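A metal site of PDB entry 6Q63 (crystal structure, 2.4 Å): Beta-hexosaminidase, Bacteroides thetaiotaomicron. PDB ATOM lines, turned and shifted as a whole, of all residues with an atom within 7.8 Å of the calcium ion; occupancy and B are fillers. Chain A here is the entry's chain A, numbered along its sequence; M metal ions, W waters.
The backbone NH of Gly 645 sits at hydrogen-bond distance from the side-chain carboxylate of Glu 770 (2.9 Å).
N of Gly 648 lies within hydrogen-bond range of OD2 of Asp 769, at 2.9 Å.
The side-chain carboxylate of Asp 769 lies within salt-bridge range of the side-chain amino group of Lys 647 (3.1 Å).
Of the 18 residues printed, 5 come within 4 Å of the calcium ion.
Along chain A the residues within 4 Å of the calcium ion span positions 641 to 770.
The calcium ion is bound by O of Leu 646, at 2.2 Å.
The calcium ion is bound by OE1 of Glu 770.
O of Thr 641 binds the calcium ion (2.3 Å).
The calcium ion is bound by O of Asp 769, 2.4 Å away.
OD1 of Asp 644 binds the calcium ion (2.4 Å).
The calcium ion is bound by water W1 (2.4 Å).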
ATOM      1  N   ASP A 615      -3.970  -4.594   3.816  1.00  0.00           N
ATOM      2  CA  ASP A 615      -4.680  -5.900   3.959  1.00  0.00           C
ATOM      3  C   ASP A 615      -5.960  -5.656   4.761  1.00  0.00           C
ATOM      4  O   ASP A 615      -5.942  -5.857   5.990  1.00  0.00           O
ATOM      5  CB  ASP A 615      -3.755  -6.931   4.621  1.00  0.00           C
ATOM      6  CG  ASP A 615      -3.951  -8.362   4.146  1.00  0.00           C
ATOM      7  OD1 ASP A 615      -5.085  -8.720   3.763  1.00  0.00           O
ATOM      8  OD2 ASP A 615      -2.947  -9.115   4.172  1.00  0.00           O
ATOM      9  N   VAL A 639      -2.622  -3.389  21.134  1.00  0.00           N
ATOM     10  CA  VAL A 639      -3.430  -4.442  20.455  1.00  0.00           C
ATOM     11  C   VAL A 639      -4.045  -3.908  19.155  1.00  0.00           C
ATOM     12  O   VAL A 639      -4.259  -4.721  18.228  1.00  0.00           O
ATOM     13  CB  VAL A 639      -4.522  -5.027  21.372  1.00  0.00           C
ATOM     14  CG1 VAL A 639      -3.959  -6.063  22.324  1.00  0.00           C
ATOM     15  CG2 VAL A 639      -5.292  -3.951  22.123  1.00  0.00           C
ATOM     16  N   SER A 640      -4.332  -2.608  19.081  1.00  0.00           N
ATOM     17  CA  SER A 640      -4.933  -1.926  17.903  1.00  0.00           C
ATOM     18  C   SER A 640      -4.045  -2.123  16.659  1.00  0.00           C
ATOM     19  O   SER A 640      -4.575  -1.977  15.542  1.00  0.00           O
ATOM     20  CB  SER A 640      -5.201  -0.465  18.186  1.00  0.00           C
ATOM     21  OG  SER A 640      -4.120   0.117  18.900  1.00  0.00           O
ATOM     22  N   THR A 641      -2.762  -2.443  16.846  1.00  0.00           N
ATOM     23  CA  THR A 641      -1.764  -2.733  15.777  1.00  0.00           C
ATOM     24  C   THR A 641      -2.188  -3.975  14.954  1.00  0.00           C
ATOM     25  O   THR A 641      -1.779  -4.056  13.766  1.00  0.00           O
ATOM     26  CB  THR A 641      -0.357  -2.951  16.364  1.00  0.00           C
ATOM     27  OG1 THR A 641      -0.041  -1.837  17.203  1.00  0.00           O
ATOM     28  CG2 THR A 641       0.714  -3.110  15.308  1.00  0.00           C
ATOM     29  N   LEU A 642      -2.961  -4.889  15.553  1.00  0.00           N
ATOM     30  CA  LEU A 642      -3.332  -6.193  14.935  1.00  0.00           C
ATOM     31  C   LEU A 642      -4.545  -6.046  13.997  1.00  0.00           C
ATOM     32  O   LEU A 642      -4.896  -7.045  13.345  1.00  0.00           O
ATOM     33  CB  LEU A 642      -3.629  -7.204  16.052  1.00  0.00           C
ATOM     34  CG  LEU A 642      -2.472  -7.492  17.007  1.00  0.00           C
ATOM     35  CD1 LEU A 642      -2.949  -8.331  18.181  1.00  0.00           C
ATOM     36  CD2 LEU A 642      -1.327  -8.184  16.290  1.00  0.00           C
ATOM     37  N   VAL A 643      -5.169  -4.862  13.923  1.00  0.00           N
ATOM     38  CA  VAL A 643      -6.391  -4.607  13.089  1.00  0.00           C
ATOM     39  C   VAL A 643      -6.287  -3.240  12.392  1.00  0.00           C
ATOM     40  O   VAL A 643      -7.345  -2.585  12.231  1.00  0.00           O
ATOM     41  CB  VAL A 643      -7.677  -4.717  13.927  1.00  0.00           C
ATOM     42  CG1 VAL A 643      -7.882  -6.131  14.455  1.00  0.00           C
ATOM     43  CG2 VAL A 643      -7.708  -3.719  15.073  1.00  0.00           C
ATOM     44  N   ASP A 644      -5.088  -2.822  11.976  1.00  0.00           N
ATOM     45  CA  ASP A 644      -4.871  -1.521  11.295  1.00  0.00           C
ATOM     46  C   ASP A 644      -4.710  -1.729   9.774  1.00  0.00           C
ATOM     47  O   ASP A 644      -4.554  -0.725   9.061  1.00  0.00           O
ATOM     48  CB  ASP A 644      -3.688  -0.755  11.901  1.00  0.00           C
ATOM     49  CG  ASP A 644      -2.338  -1.437  11.810  1.00  0.00           C
ATOM     50  OD1 ASP A 644      -2.204  -2.432  11.068  1.00  0.00           O
ATOM     51  OD2 ASP A 644      -1.403  -0.948  12.484  1.00  0.00           O
ATOM     52  N   GLY A 645      -4.745  -2.984   9.307  1.00  0.00           N
ATOM     53  CA  GLY A 645      -4.594  -3.337   7.878  1.00  0.00           C
ATOM     54  C   GLY A 645      -3.138  -3.344   7.426  1.00  0.00           C
ATOM     55  O   GLY A 645      -2.901  -3.664   6.240  1.00  0.00           O
ATOM     56  N   LEU A 646      -2.182  -3.015   8.304  1.00  0.00           N
ATOM     57  CA  LEU A 646      -0.738  -2.970   7.981  1.00  0.00           C
ATOM     58  C   LEU A 646      -0.079  -4.286   8.398  1.00  0.00           C
ATOM     59  O   LEU A 646      -0.416  -4.795   9.488  1.00  0.00           O
ATOM     60  CB  LEU A 646      -0.080  -1.789   8.695  1.00  0.00           C
ATOM     61  CG  LEU A 646      -0.660  -0.417   8.370  1.00  0.00           C
ATOM     62  CD1 LEU A 646      -0.027   0.655   9.254  1.00  0.00           C
ATOM     63  CD2 LEU A 646      -0.457  -0.076   6.902  1.00  0.00           C
ATOM     64  N   LYS A 647       0.834  -4.796   7.567  1.00  0.00           N
ATOM     65  CA  LYS A 647       1.656  -6.015   7.831  1.00  0.00           C
ATOM     66  C   LYS A 647       3.116  -5.582   8.034  1.00  0.00           C
ATOM     67  O   LYS A 647       3.479  -4.489   7.549  1.00  0.00           O
ATOM     68  CB  LYS A 647       1.514  -6.996   6.660  1.00  0.00           C
ATOM     69  CG  LYS A 647       0.095  -7.452   6.372  1.00  0.00           C
ATOM     70  CD  LYS A 647      -0.415  -8.483   7.357  1.00  0.00           C
ATOM     71  CE  LYS A 647       0.094  -9.881   7.065  1.00  0.00           C
ATOM     72  NZ  LYS A 647      -0.050 -10.787   8.226  1.00  0.00           N
ATOM     73  N   GLY A 648       3.904  -6.399   8.723  1.00  0.00           N
ATOM     74  CA  GLY A 648       5.337  -6.150   8.984  1.00  0.00           C
ATOM     75  C   GLY A 648       6.220  -6.965   8.059  1.00  0.00           C
ATOM     76  O   GLY A 648       5.671  -7.747   7.247  1.00  0.00           O
ATOM     77  N   GLY A 655       7.464  -1.517  14.862  1.00  0.00           N
ATOM     78  CA  GLY A 655       6.172  -1.117  15.457  1.00  0.00           C
ATOM     79  C   GLY A 655       4.990  -1.718  14.707  1.00  0.00           C
ATOM     80  O   GLY A 655       3.843  -1.528  15.159  1.00  0.00           O
ATOM     81  N   ARG A 656       5.269  -2.422  13.606  1.00  0.00           N
ATOM     82  CA  ARG A 656       4.272  -3.218  12.842  1.00  0.00           C
ATOM     83  C   ARG A 656       3.958  -4.516  13.609  1.00  0.00           C
ATOM     84  O   ARG A 656       2.848  -5.062  13.403  1.00  0.00           O
ATOM     85  CB  ARG A 656       4.796  -3.521  11.437  1.00  0.00           C
ATOM     86  CG  ARG A 656       4.917  -2.297  10.538  1.00  0.00           C
ATOM     87  CD  ARG A 656       3.568  -1.680  10.244  1.00  0.00           C
ATOM     88  NE  ARG A 656       3.672  -0.411   9.541  1.00  0.00           N
ATOM     89  CZ  ARG A 656       3.843  -0.284   8.220  1.00  0.00           C
ATOM     90  NH1 ARG A 656       3.925  -1.351   7.452  1.00  0.00           N
ATOM     91  NH2 ARG A 656       3.917   0.921   7.681  1.00  0.00           N
ATOM     92  N   TRP A 657       4.880  -4.971  14.458  1.00  0.00           N
ATOM     93  CA  TRP A 657       4.749  -6.176  15.305  1.00  0.00           C
ATOM     94  C   TRP A 657       4.635  -5.772  16.777  1.00  0.00           C
ATOM     95  O   TRP A 657       5.391  -4.874  17.200  1.00  0.00           O
ATOM     96  CB  TRP A 657       5.957  -7.110  15.120  1.00  0.00           C
ATOM     97  CG  TRP A 657       6.273  -7.430  13.698  1.00  0.00           C
ATOM     98  CD1 TRP A 657       7.066  -6.721  12.849  1.00  0.00           C
ATOM     99  CD2 TRP A 657       5.813  -8.575  12.948  1.00  0.00           C
ATOM    100  NE1 TRP A 657       7.136  -7.337  11.626  1.00  0.00           N
ATOM    101  CE2 TRP A 657       6.374  -8.468  11.660  1.00  0.00           C
ATOM    102  CE3 TRP A 657       4.989  -9.667  13.253  1.00  0.00           C
ATOM    103  CZ2 TRP A 657       6.133  -9.420  10.662  1.00  0.00           C
ATOM    104  CZ3 TRP A 657       4.745 -10.603  12.261  1.00  0.00           C
ATOM    105  CH2 TRP A 657       5.308 -10.477  10.988  1.00  0.00           C
ATOM    106  N   VAL A 768       3.446 -10.741  16.451  1.00  0.00           N
ATOM    107  CA  VAL A 768       2.267 -10.815  15.531  1.00  0.00           C
ATOM    108  C   VAL A 768       1.992  -9.400  15.001  1.00  0.00           C
ATOM    109  O   VAL A 768       2.091  -8.440  15.805  1.00  0.00           O
ATOM    110  CB  VAL A 768       1.040 -11.415  16.235  1.00  0.00           C
ATOM    111  CG1 VAL A 768      -0.114 -11.654  15.265  1.00  0.00           C
ATOM    112  CG2 VAL A 768       1.368 -12.697  16.982  1.00  0.00           C
ATOM    113  N   ASP A 769       1.636  -9.274  13.717  1.00  0.00           N
ATOM    114  CA  ASP A 769       1.485  -7.970  13.025  1.00  0.00           C
ATOM    115  C   ASP A 769       0.018  -7.666  12.687  1.00  0.00           C
ATOM    116  O   ASP A 769      -0.330  -6.477  12.682  1.00  0.00           O
ATOM    117  CB  ASP A 769       2.343  -7.904  11.754  1.00  0.00           C
ATOM    118  CG  ASP A 769       1.994  -8.909  10.678  1.00  0.00           C
ATOM    119  OD1 ASP A 769       1.200  -9.835  10.956  1.00  0.00           O
ATOM    120  OD2 ASP A 769       2.527  -8.760   9.556  1.00  0.00           O
ATOM    121  N   GLU A 770      -0.793  -8.687  12.396  1.00  0.00           N
ATOM    122  CA  GLU A 770      -2.171  -8.490  11.888  1.00  0.00           C
ATOM    123  C   GLU A 770      -3.001  -9.772  12.084  1.00  0.00           C
ATOM    124  O   GLU A 770      -2.462 -10.876  11.867  1.00  0.00           O
ATOM    125  CB  GLU A 770      -2.138  -8.088  10.412  1.00  0.00           C
ATOM    126  CG  GLU A 770      -3.465  -7.570   9.871  1.00  0.00           C
ATOM    127  CD  GLU A 770      -3.905  -6.201  10.370  1.00  0.00           C
ATOM    128  OE1 GLU A 770      -3.107  -5.533  11.051  1.00  0.00           O
ATOM    129  OE2 GLU A 770      -5.043  -5.804  10.072  1.00  0.00           O
ATOM    130  N   ILE A 771      -4.268  -9.599  12.474  1.00  0.00           N
ATOM    131  CA  ILE A 771      -5.327 -10.653  12.474  1.00  0.00           C
ATOM    132  C   ILE A 771      -6.310 -10.312  11.356  1.00  0.00           C
ATOM    133  O   ILE A 771      -7.066  -9.336  11.501  1.00  0.00           O
ATOM    134  CB  ILE A 771      -6.002 -10.749  13.855  1.00  0.00           C
ATOM    135  CG1 ILE A 771      -4.999 -11.065  14.964  1.00  0.00           C
ATOM    136  CG2 ILE A 771      -7.137 -11.768  13.819  1.00  0.00           C
ATOM    137  CD1 ILE A 771      -5.531 -10.880  16.365  1.00  0.00           C
HETATM  138 CA    CA M   1      -1.112  -4.518  11.602  1.00  0.00          CA
HETATM  139  O   HOH W   1       1.070  -3.567  12.083  1.00  0.00           O
